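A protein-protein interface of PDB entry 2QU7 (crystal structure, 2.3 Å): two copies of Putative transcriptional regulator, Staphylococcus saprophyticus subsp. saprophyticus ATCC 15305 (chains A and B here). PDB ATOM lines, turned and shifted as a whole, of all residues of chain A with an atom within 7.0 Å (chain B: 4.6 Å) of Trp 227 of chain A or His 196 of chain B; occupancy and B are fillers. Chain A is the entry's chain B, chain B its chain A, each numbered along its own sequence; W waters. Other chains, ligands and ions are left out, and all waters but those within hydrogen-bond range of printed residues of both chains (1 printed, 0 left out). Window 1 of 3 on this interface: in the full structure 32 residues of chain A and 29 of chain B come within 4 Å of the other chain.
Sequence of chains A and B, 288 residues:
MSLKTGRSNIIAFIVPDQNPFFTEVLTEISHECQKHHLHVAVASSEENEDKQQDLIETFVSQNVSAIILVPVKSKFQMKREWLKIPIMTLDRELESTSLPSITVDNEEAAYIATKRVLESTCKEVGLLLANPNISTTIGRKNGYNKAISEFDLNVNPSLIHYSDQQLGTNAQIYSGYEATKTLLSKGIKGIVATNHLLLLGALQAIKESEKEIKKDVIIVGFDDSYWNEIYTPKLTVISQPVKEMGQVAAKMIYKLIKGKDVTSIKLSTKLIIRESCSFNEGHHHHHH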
ATOM      1  N   HIS A 196       1.872  13.455  34.691  1.00  0.00           N
ATOM      2  CA  HIS A 196       1.163  12.379  33.982  1.00  0.00           C
ATOM      3  C   HIS A 196       0.130  11.674  34.856  1.00  0.00           C
ATOM      4  O   HIS A 196      -1.015  11.478  34.452  1.00  0.00           O
ATOM      5  CB  HIS A 196       2.184  11.381  33.402  1.00  0.00           C
ATOM      6  CG  HIS A 196       1.568  10.350  32.510  1.00  0.00           C
ATOM      7  ND1 HIS A 196       1.245  10.604  31.193  1.00  0.00           N
ATOM      8  CD2 HIS A 196       1.204   9.066  32.749  1.00  0.00           C
ATOM      9  CE1 HIS A 196       0.702   9.523  30.662  1.00  0.00           C
ATOM     10  NE2 HIS A 196       0.673   8.573  31.582  1.00  0.00           N
ATOM     11  N   LEU A 200      -3.857  11.462  34.653  1.00  0.00           N
ATOM     12  CA  LEU A 200      -4.672  10.214  34.603  1.00  0.00           C
ATOM     13  C   LEU A 200      -5.798  10.218  35.626  1.00  0.00           C
ATOM     14  O   LEU A 200      -6.898   9.757  35.340  1.00  0.00           O
ATOM     15  CB  LEU A 200      -3.819   8.941  34.762  1.00  0.00           C
ATOM     16  CG  LEU A 200      -2.864   8.515  33.618  1.00  0.00           C
ATOM     17  CD1 LEU A 200      -1.683   7.674  34.134  1.00  0.00           C
ATOM     18  CD2 LEU A 200      -3.578   7.809  32.397  1.00  0.00           C
ATOM     19  N   ASP A 224       4.077  13.749  27.976  1.00  0.00           N
ATOM     20  CA  ASP A 224       3.420  13.213  26.790  1.00  0.00           C
ATOM     21  C   ASP A 224       3.437  11.687  26.819  1.00  0.00           C
ATOM     22  O   ASP A 224       4.253  11.073  27.524  1.00  0.00           O
ATOM     23  CB  ASP A 224       4.055  13.769  25.499  1.00  0.00           C
ATOM     24  CG  ASP A 224       3.010  14.065  24.384  1.00  0.00           C
ATOM     25  OD1 ASP A 224       1.795  13.766  24.511  1.00  0.00           O
ATOM     26  OD2 ASP A 224       3.432  14.610  23.351  1.00  0.00           O
ATOM     27  N   SER A 225       2.488  11.108  26.088  1.00  0.00           N
ATOM     28  CA  SER A 225       2.376   9.684  25.832  1.00  0.00           C
ATOM     29  C   SER A 225       1.697   9.458  24.483  1.00  0.00           C
ATOM     30  O   SER A 225       0.889  10.292  24.045  1.00  0.00           O
ATOM     31  CB  SER A 225       1.519   9.009  26.880  1.00  0.00           C
ATOM     32  OG  SER A 225       0.998   7.817  26.315  1.00  0.00           O
ATOM     33  N   TYR A 226       2.002   8.321  23.832  1.00  0.00           N
ATOM     34  CA  TYR A 226       1.330   7.943  22.568  1.00  0.00           C
ATOM     35  C   TYR A 226      -0.190   7.901  22.754  1.00  0.00           C
ATOM     36  O   TYR A 226      -0.928   8.154  21.807  1.00  0.00           O
ATOM     37  CB  TYR A 226       1.858   6.608  21.989  1.00  0.00           C
ATOM     38  CG  TYR A 226       3.306   6.671  21.527  1.00  0.00           C
ATOM     39  CD1 TYR A 226       3.708   7.579  20.519  1.00  0.00           C
ATOM     40  CD2 TYR A 226       4.281   5.850  22.104  1.00  0.00           C
ATOM     41  CE1 TYR A 226       5.045   7.648  20.090  1.00  0.00           C
ATOM     42  CE2 TYR A 226       5.614   5.912  21.686  1.00  0.00           C
ATOM     43  CZ  TYR A 226       5.986   6.808  20.680  1.00  0.00           C
ATOM     44  OH  TYR A 226       7.299   6.877  20.273  1.00  0.00           O
ATOM     45  N   TRP A 227      -0.630   7.614  23.975  1.00  0.00           N
ATOM     46  CA  TRP A 227      -2.036   7.605  24.323  1.00  0.00           C
ATOM     47  C   TRP A 227      -2.776   8.963  24.295  1.00  0.00           C
ATOM     48  O   TRP A 227      -3.995   8.980  24.157  1.00  0.00           O
ATOM     49  CB  TRP A 227      -2.225   6.942  25.677  1.00  0.00           C
ATOM     50  CG  TRP A 227      -2.022   5.457  25.618  1.00  0.00           C
ATOM     51  CD1 TRP A 227      -0.842   4.780  25.800  1.00  0.00           C
ATOM     52  CD2 TRP A 227      -3.013   4.463  25.312  1.00  0.00           C
ATOM     53  NE1 TRP A 227      -1.041   3.429  25.641  1.00  0.00           N
ATOM     54  CE2 TRP A 227      -2.360   3.202  25.343  1.00  0.00           C
ATOM     55  CE3 TRP A 227      -4.389   4.511  25.023  1.00  0.00           C
ATOM     56  CZ2 TRP A 227      -3.036   1.998  25.087  1.00  0.00           C
ATOM     57  CZ3 TRP A 227      -5.061   3.325  24.783  1.00  0.00           C
ATOM     58  CH2 TRP A 227      -4.381   2.079  24.815  1.00  0.00           C
ATOM     59  N   ASN A 228      -2.056  10.075  24.459  1.00  0.00           N
ATOM     60  CA  ASN A 228      -2.636  11.419  24.327  1.00  0.00           C
ATOM     61  C   ASN A 228      -3.147  11.709  22.923  1.00  0.00           C
ATOM     62  O   ASN A 228      -4.143  12.395  22.769  1.00  0.00           O
ATOM     63  CB  ASN A 228      -1.616  12.506  24.705  1.00  0.00           C
ATOM     64  CG  ASN A 228      -1.173  12.434  26.164  1.00  0.00           C
ATOM     65  OD1 ASN A 228      -1.919  11.992  27.032  1.00  0.00           O
ATOM     66  ND2 ASN A 228       0.036  12.901  26.434  1.00  0.00           N
ATOM     67  N   GLU A 229      -2.454  11.195  21.903  1.00  0.00           N
ATOM     68  CA  GLU A 229      -2.836  11.393  20.498  1.00  0.00           C
ATOM     69  C   GLU A 229      -4.037  10.548  20.091  1.00  0.00           C
ATOM     70  O   GLU A 229      -4.699  10.855  19.105  1.00  0.00           O
ATOM     71  CB  GLU A 229      -1.684  11.048  19.544  1.00  0.00           C
ATOM     72  CG  GLU A 229      -0.469  11.980  19.605  1.00  0.00           C
ATOM     73  CD  GLU A 229       0.789  11.389  18.954  1.00  0.00           C
ATOM     74  OE1 GLU A 229       1.838  12.071  18.989  1.00  0.00           O
ATOM     75  OE2 GLU A 229       0.744  10.242  18.422  1.00  0.00           O
ATOM     76  N   ILE A 230      -4.307   9.474  20.822  1.00  0.00           N
ATOM     77  CA  ILE A 230      -5.441   8.626  20.473  1.00  0.00           C
ATOM     78  C   ILE A 230      -6.590   8.745  21.467  1.00  0.00           C
ATOM     79  O   ILE A 230      -7.657   8.145  21.269  1.00  0.00           O
ATOM     80  CB  ILE A 230      -5.044   7.121  20.213  1.00  0.00           C
ATOM     81  CG1 ILE A 230      -4.291   6.519  21.397  1.00  0.00           C
ATOM     82  CG2 ILE A 230      -4.224   6.986  18.943  1.00  0.00           C
ATOM     83  CD1 ILE A 230      -4.342   4.996  21.417  1.00  0.00           C
ATOM     84  N   TYR A 231      -6.386   9.517  22.536  1.00  0.00           N
ATOM     85  CA  TYR A 231      -7.485   9.816  23.459  1.00  0.00           C
ATOM     86  C   TYR A 231      -8.597  10.615  22.766  1.00  0.00           C
ATOM     87  O   TYR A 231      -8.333  11.330  21.817  1.00  0.00           O
ATOM     88  CB  TYR A 231      -6.992  10.607  24.663  1.00  0.00           C
ATOM     89  CG  TYR A 231      -7.881  10.435  25.862  1.00  0.00           C
ATOM     90  CD1 TYR A 231      -7.819   9.279  26.628  1.00  0.00           C
ATOM     91  CD2 TYR A 231      -8.794  11.432  26.236  1.00  0.00           C
ATOM     92  CE1 TYR A 231      -8.638   9.111  27.741  1.00  0.00           C
ATOM     93  CE2 TYR A 231      -9.619  11.273  27.350  1.00  0.00           C
ATOM     94  CZ  TYR A 231      -9.521  10.108  28.099  1.00  0.00           C
ATOM     95  OH  TYR A 231     -10.328   9.917  29.192  1.00  0.00           O
ATOM     96  N   THR A 232      -9.826  10.474  23.251  1.00  0.00           N
ATOM     97  CA  THR A 232     -10.944  11.309  22.816  1.00  0.00           C
ATOM     98  C   THR A 232     -11.400  12.241  23.949  1.00  0.00           C
ATOM     99  O   THR A 232     -11.979  11.772  24.935  1.00  0.00           O
ATOM    100  CB  THR A 232     -12.154  10.474  22.371  1.00  0.00           C
ATOM    101  OG1 THR A 232     -11.725   9.503  21.408  1.00  0.00           O
ATOM    102  CG2 THR A 232     -13.258  11.376  21.776  1.00  0.00           C
ATOM    103  N   PRO A 233     -11.161  13.566  23.795  1.00  0.00           N
ATOM    104  CA  PRO A 233     -10.478  14.143  22.653  1.00  0.00           C
ATOM    105  C   PRO A 233      -8.971  14.056  22.879  1.00  0.00           C
ATOM    106  O   PRO A 233      -8.537  13.673  23.969  1.00  0.00           O
ATOM    107  CB  PRO A 233     -10.948  15.603  22.683  1.00  0.00           C
ATOM    108  CG  PRO A 233     -11.134  15.897  24.126  1.00  0.00           C
ATOM    109  CD  PRO A 233     -11.568  14.602  24.769  1.00  0.00           C
ATOM    110  N   LYS A 234      -8.190  14.379  21.855  1.00  0.00           N
ATOM    111  CA  LYS A 234      -6.758  14.362  21.969  1.00  0.00           C
ATOM    112  C   LYS A 234      -6.304  15.371  23.013  1.00  0.00           C
ATOM    113  O   LYS A 234      -6.843  16.501  23.113  1.00  0.00           O
ATOM    114  CB  LYS A 234      -6.123  14.672  20.628  1.00  0.00           C
ATOM    115  CG  LYS A 234      -6.517  13.696  19.522  1.00  0.00           C
ATOM    116  CD  LYS A 234      -5.867  14.094  18.226  1.00  0.00           C
ATOM    117  CE  LYS A 234      -6.255  13.158  17.098  1.00  0.00           C
ATOM    118  NZ  LYS A 234      -5.496  13.553  15.872  1.00  0.00           N
ATOM    119  N   LEU A 235      -5.283  14.970  23.767  1.00  0.00           N
ATOM    120  CA  LEU A 235      -4.866  15.691  24.953  1.00  0.00           C
ATOM    121  C   LEU A 235      -3.716  16.651  24.702  1.00  0.00           C
ATOM    122  O   LEU A 235      -2.648  16.269  24.219  1.00  0.00           O
ATOM    123  CB  LEU A 235      -4.508  14.685  26.053  1.00  0.00           C
ATOM    124  CG  LEU A 235      -5.665  13.756  26.439  1.00  0.00           C
ATOM    125  CD1 LEU A 235      -5.173  12.652  27.368  1.00  0.00           C
ATOM    126  CD2 LEU A 235      -6.848  14.517  27.081  1.00  0.00           C
ATOM    127  N   ASN B  19       6.638  -2.456  28.557  1.00  0.00           N
ATOM    128  CA  ASN B  19       5.231  -2.764  28.790  1.00  0.00           C
ATOM    129  C   ASN B  19       4.904  -2.533  30.286  1.00  0.00           C
ATOM    130  O   ASN B  19       5.550  -3.131  31.163  1.00  0.00           O
ATOM    131  CB  ASN B  19       4.965  -4.216  28.352  1.00  0.00           C
ATOM    132  CG  ASN B  19       3.486  -4.636  28.447  1.00  0.00           C
ATOM    133  OD1 ASN B  19       2.688  -4.027  29.153  1.00  0.00           O
ATOM    134  ND2 ASN B  19       3.132  -5.717  27.735  1.00  0.00           N
ATOM    135  N   PRO B  20       3.917  -1.659  30.590  1.00  0.00           N
ATOM    136  CA  PRO B  20       3.483  -1.392  31.976  1.00  0.00           C
ATOM    137  C   PRO B  20       3.193  -2.657  32.768  1.00  0.00           C
ATOM    138  O   PRO B  20       3.175  -2.630  33.986  1.00  0.00           O
ATOM    139  CB  PRO B  20       2.169  -0.606  31.794  1.00  0.00           C
ATOM    140  CG  PRO B  20       1.812  -0.748  30.317  1.00  0.00           C
ATOM    141  CD  PRO B  20       3.138  -0.840  29.640  1.00  0.00           C
ATOM    142  N   ASN B 195      -0.886  -8.111  23.439  1.00  0.00           N
ATOM    143  CA  ASN B 195      -0.216  -7.372  24.512  1.00  0.00           C
ATOM    144  C   ASN B 195      -0.503  -5.874  24.391  1.00  0.00           C
ATOM    145  O   ASN B 195      -1.023  -5.422  23.375  1.00  0.00           O
ATOM    146  CB  ASN B 195       1.280  -7.741  24.670  1.00  0.00           C
ATOM    147  CG  ASN B 195       2.210  -7.050  23.655  1.00  0.00           C
ATOM    148  OD1 ASN B 195       2.025  -5.886  23.289  1.00  0.00           O
ATOM    149  ND2 ASN B 195       3.255  -7.773  23.237  1.00  0.00           N
ATOM    150  N   HIS B 196      -0.190  -5.128  25.442  1.00  0.00           N
ATOM    151  CA  HIS B 196      -0.528  -3.716  25.557  1.00  0.00           C
ATOM    152  C   HIS B 196       0.113  -2.852  24.468  1.00  0.00           C
ATOM    153  O   HIS B 196      -0.478  -1.886  23.981  1.00  0.00           O
ATOM    154  CB  HIS B 196      -0.115  -3.214  26.967  1.00  0.00           C
ATOM    155  CG  HIS B 196      -0.306  -1.745  27.167  1.00  0.00           C
ATOM    156  ND1 HIS B 196      -1.476  -1.207  27.661  1.00  0.00           N
ATOM    157  CD2 HIS B 196       0.530  -0.700  26.947  1.00  0.00           C
ATOM    158  CE1 HIS B 196      -1.350   0.107  27.739  1.00  0.00           C
ATOM    159  NE2 HIS B 196      -0.140   0.442  27.316  1.00  0.00           N
ATOM    160  N   LEU B 197       1.342  -3.194  24.110  1.00  0.00           N
ATOM    161  CA  LEU B 197       2.065  -2.479  23.064  1.00  0.00           C
ATOM    162  C   LEU B 197       1.452  -2.691  21.676  1.00  0.00           C
ATOM    163  O   LEU B 197       1.274  -1.742  20.932  1.00  0.00           O
ATOM    164  CB  LEU B 197       3.554  -2.847  23.091  1.00  0.00           C
ATOM    165  CG  LEU B 197       4.244  -2.587  24.438  1.00  0.00           C
ATOM    166  CD1 LEU B 197       5.734  -2.998  24.381  1.00  0.00           C
ATOM    167  CD2 LEU B 197       4.097  -1.102  24.857  1.00  0.00           C
ATOM    168  N   LEU B 198       1.096  -3.933  21.348  1.00  0.00           N
ATOM    169  CA  LEU B 198       0.408  -4.222  20.072  1.00  0.00           C
ATOM    170  C   LEU B 198      -0.955  -3.550  20.046  1.00  0.00           C
ATOM    171  O   LEU B 198      -1.371  -3.044  19.002  1.00  0.00           O
ATOM    172  CB  LEU B 198       0.273  -5.747  19.813  1.00  0.00           C
ATOM    173  CG  LEU B 198       1.602  -6.499  19.752  1.00  0.00           C
ATOM    174  CD1 LEU B 198       1.441  -8.025  19.937  1.00  0.00           C
ATOM    175  CD2 LEU B 198       2.399  -6.161  18.476  1.00  0.00           C
ATOM    176  N   LEU B 199      -1.636  -3.549  21.196  1.00  0.00           N
ATOM    177  CA  LEU B 199      -2.942  -2.875  21.361  1.00  0.00           C
ATOM    178  C   LEU B 199      -2.850  -1.383  21.045  1.00  0.00           C
ATOM    179  O   LEU B 199      -3.621  -0.865  20.224  1.00  0.00           O
ATOM    180  CB  LEU B 199      -3.506  -3.081  22.783  1.00  0.00           C
ATOM    181  CG  LEU B 199      -4.775  -2.297  23.209  1.00  0.00           C
ATOM    182  CD1 LEU B 199      -6.047  -2.631  22.365  1.00  0.00           C
ATOM    183  CD2 LEU B 199      -5.069  -2.478  24.687  1.00  0.00           C
ATOM    184  N   LEU B 200      -1.903  -0.707  21.692  1.00  0.00           N
ATOM    185  CA  LEU B 200      -1.614   0.698  21.413  1.00  0.00           C
ATOM    186  C   LEU B 200      -1.375   0.959  19.923  1.00  0.00           C
ATOM    187  O   LEU B 200      -1.960   1.872  19.360  1.00  0.00           O
ATOM    188  CB  LEU B 200      -0.399   1.155  22.212  1.00  0.00           C
ATOM    189  CG  LEU B 200       0.185   2.536  21.927  1.00  0.00           C
ATOM    190  CD1 LEU B 200      -0.864   3.649  22.094  1.00  0.00           C
ATOM    191  CD2 LEU B 200       1.383   2.777  22.855  1.00  0.00           C
ATOM    192  N   LEU B 203      -4.721   0.630  18.081  1.00  0.00           N
ATOM    193  CA  LEU B 203      -5.575   1.777  18.329  1.00  0.00           C
ATOM    194  C   LEU B 203      -5.132   3.000  17.525  1.00  0.00           C
ATOM    195  O   LEU B 203      -5.981   3.712  16.996  1.00  0.00           O
ATOM    196  CB  LEU B 203      -5.633   2.077  19.816  1.00  0.00           C
ATOM    197  CG  LEU B 203      -6.301   0.973  20.652  1.00  0.00           C
ATOM    198  CD1 LEU B 203      -6.132   1.248  22.110  1.00  0.00           C
ATOM    199  CD2 LEU B 203      -7.769   0.813  20.313  1.00  0.00           C
ATOM    200  N   PHE B 222      -4.822  -7.171  25.398  1.00  0.00           N
ATOM    201  CA  PHE B 222      -4.250  -7.822  26.549  1.00  0.00           C
ATOM    202  C   PHE B 222      -3.642  -6.758  27.440  1.00  0.00           C
ATOM    203  O   PHE B 222      -3.114  -5.764  26.948  1.00  0.00           O
ATOM    204  CB  PHE B 222      -3.146  -8.791  26.107  1.00  0.00           C
ATOM    205  CG  PHE B 222      -3.623 -10.206  25.853  1.00  0.00           C
ATOM    206  CD1 PHE B 222      -4.623 -10.475  24.917  1.00  0.00           C
ATOM    207  CD2 PHE B 222      -3.054 -11.275  26.548  1.00  0.00           C
ATOM    208  CE1 PHE B 222      -5.040 -11.796  24.690  1.00  0.00           C
ATOM    209  CE2 PHE B 222      -3.471 -12.562  26.340  1.00  0.00           C
ATOM    210  CZ  PHE B 222      -4.450 -12.834  25.411  1.00  0.00           C
ATOM    211  N   ASP B 223      -3.702  -6.983  28.745  1.00  0.00           N
ATOM    212  CA  ASP B 223      -2.916  -6.226  29.743  1.00  0.00           C
ATOM    213  C   ASP B 223      -3.742  -5.066  30.290  1.00  0.00           C
ATOM    214  O   ASP B 223      -4.252  -4.223  29.532  1.00  0.00           O
ATOM    215  CB  ASP B 223      -1.591  -5.685  29.204  1.00  0.00           C
ATOM    216  CG  ASP B 223      -0.611  -6.776  28.754  1.00  0.00           C
ATOM    217  OD1 ASP B 223      -0.733  -7.925  29.230  1.00  0.00           O
ATOM    218  OD2 ASP B 223       0.328  -6.465  27.956  1.00  0.00           O
ATOM    219  N   SER B 225      -4.371  -1.602  32.079  1.00  0.00           N
ATOM    220  CA  SER B 225      -3.817  -0.254  31.996  1.00  0.00           C
ATOM    221  C   SER B 225      -4.890   0.740  32.410  1.00  0.00           C
ATOM    222  O   SER B 225      -6.109   0.488  32.249  1.00  0.00           O
ATOM    223  CB  SER B 225      -3.368   0.073  30.567  1.00  0.00           C
ATOM    224  OG  SER B 225      -2.913   1.415  30.485  1.00  0.00           O
ATOM    225  N   TRP B 227      -5.331   3.537  31.016  1.00  0.00           N
ATOM    226  CA  TRP B 227      -5.906   3.967  29.740  1.00  0.00           C
ATOM    227  C   TRP B 227      -7.220   3.237  29.402  1.00  0.00           C
ATOM    228  O   TRP B 227      -8.086   3.832  28.778  1.00  0.00           O
ATOM    229  CB  TRP B 227      -4.879   3.825  28.588  1.00  0.00           C
ATOM    230  CG  TRP B 227      -3.681   4.767  28.716  1.00  0.00           C
ATOM    231  CD1 TRP B 227      -2.379   4.417  28.922  1.00  0.00           C
ATOM    232  CD2 TRP B 227      -3.702   6.208  28.657  1.00  0.00           C
ATOM    233  NE1 TRP B 227      -1.586   5.541  28.988  1.00  0.00           N
ATOM    234  CE2 TRP B 227      -2.374   6.654  28.845  1.00  0.00           C
ATOM    235  CE3 TRP B 227      -4.718   7.162  28.463  1.00  0.00           C
ATOM    236  CZ2 TRP B 227      -2.029   8.022  28.842  1.00  0.00           C
ATOM    237  CZ3 TRP B 227      -4.377   8.525  28.464  1.00  0.00           C
ATOM    238  CH2 TRP B 227      -3.039   8.938  28.648  1.00  0.00           C
ATOM    239  N   TYR B 231     -10.476   5.242  27.937  1.00  0.00           N
ATOM    240  CA  TYR B 231     -10.428   5.351  26.492  1.00  0.00           C
ATOM    241  C   TYR B 231     -11.848   5.463  25.914  1.00  0.00           C
ATOM    242  O   TYR B 231     -12.816   5.052  26.554  1.00  0.00           O
ATOM    243  CB  TYR B 231      -9.691   4.145  25.902  1.00  0.00           C
ATOM    244  CG  TYR B 231      -9.243   4.387  24.480  1.00  0.00           C
ATOM    245  CD1 TYR B 231      -8.150   5.214  24.206  1.00  0.00           C
ATOM    246  CD2 TYR B 231      -9.928   3.815  23.405  1.00  0.00           C
ATOM    247  CE1 TYR B 231      -7.745   5.458  22.901  1.00  0.00           C
ATOM    248  CE2 TYR B 231      -9.526   4.062  22.098  1.00  0.00           C
ATOM    249  CZ  TYR B 231      -8.443   4.876  21.855  1.00  0.00           C
ATOM    250  OH  TYR B 231      -8.042   5.105  20.540  1.00  0.00           O
ATOM    251  N   LEU B 235     -11.977  -0.096  26.797  1.00  0.00           N
ATOM    252  CA  LEU B 235     -11.318  -1.255  26.192  1.00  0.00           C
ATOM    253  C   LEU B 235     -11.499  -2.564  26.949  1.00  0.00           C
ATOM    254  O   LEU B 235     -11.051  -2.698  28.089  1.00  0.00           O
ATOM    255  CB  LEU B 235      -9.822  -0.969  25.941  1.00  0.00           C
ATOM    256  CG  LEU B 235      -9.533   0.220  25.016  1.00  0.00           C
ATOM    257  CD1 LEU B 235      -8.096   0.637  25.191  1.00  0.00           C
ATOM    258  CD2 LEU B 235      -9.814  -0.090  23.550  1.00  0.00           C
HETATM  259  O   HOH W   1       0.782   6.230  30.187  1.00  0.00           O
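Printed residues of chain B within 4 Å of Ser 225 of chain A: Trp 227.
Printed residues of chain B within 4 Å of Trp 227 of chain A: His 196 (3.5 Å), Leu 200 (3.6 Å), Leu 203 (3.3 Å), Trp 227 (3.2 Å) and Tyr 231 (3.7 Å).
Of chain A, only Trp 227 comes within 4 Å of His 196 of chain B.
Printed residues of chain A within 4 Å of Tyr 231 of chain B: Trp 227 (3.7 Å) and Ile 230 (3.1 Å).
Among the printed residues, merely in contact across the chains: Trp 227 of chain A with Trp 227 of chain B, Trp 227 of chain A with Leu 203 of chain B, Trp 227 of chain A with His 196 of chain B, Trp 227 of chain A with Leu 200 of chain B, Ile 230 of chain A with Leu 203 of chain B, His 196 of chain A with Trp 227 of chain B, Asn 228 of chain A with Trp 227 of chain B, Trp 227 of chain A with Tyr 231 of chain B, Ile 230 of chain A with Leu 200 of chain B, Leu 200 of chain A with Trp 227 of chain B, Ser 225 of chain A with Trp 227 of chain B, Tyr 226 of chain A with Leu 200 of chain B and Tyr 231 of chain A with Trp 227 of chain B.
Hydrophobic or aromatic side chains of chain A within 4 Å of the printed part of chain B: His 196, Leu 200, Tyr 226, Trp 227, Ile 230 and Tyr 231.
Of the 15 printed residues of chain B, 5 touch a printed residue of chain A.
Among the printed residues, 14 pairs touch across the chains.
Water W1 lies within hydrogen-bond range of NE2 of His 196 of chain A and NE1 of Trp 227 of chain B.
The backbone carbonyl oxygen (O) of Ile 230 of chain A sits close to the side-chain hydroxyl (OH) of Tyr 231 of chain B, 3.1 Å away.
His 196 of chain A touches Trp 227 of chain B, and with the chains exchanged Trp 227 of chain A touches His 196 of chain B.
Ser 225 of chain A touches Trp 227 of chain B, but with the chains exchanged Trp 227 of chain A does not touch Ser 225 of chain B (5.4 Å).
Trp 227 of chain B touches its own counterpart, Trp 227 of chain A.
Trp 227 of chain A touches Tyr 231 of chain B, and with the chains exchanged Tyr 231 of chain A touches Trp 227 of chain B.
The backbone carbonyl oxygen of Phe 222 of chain B lies within hydrogen-bond range of the backbone NH of His 196 of chain B (3.3 Å).
The side-chain carboxylate of Asp 223 of chain B is in hydrogen-bond range of the backbone NH of His 196 of chain B (2.9 Å).
The side-chain carboxylate (OD1) of Asp 224 of chain A is in hydrogen-bond range of the side-chain amide nitrogen (ND2) of Asn 228 of chain A (2.7 Å).
OG of Ser 225 of chain A sits at hydrogen-bond distance from N of Trp 227 of chain A (2.9 Å).
ND2 of Asn 228 of chain A sits close to N of Ser 225 of chain A, at 3.1 Å.
The backbone carbonyl oxygen (O) of Asn 228 of chain A is in hydrogen-bond range of the backbone NH (N) of Leu 235 of chain A, 3.0 Å away.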
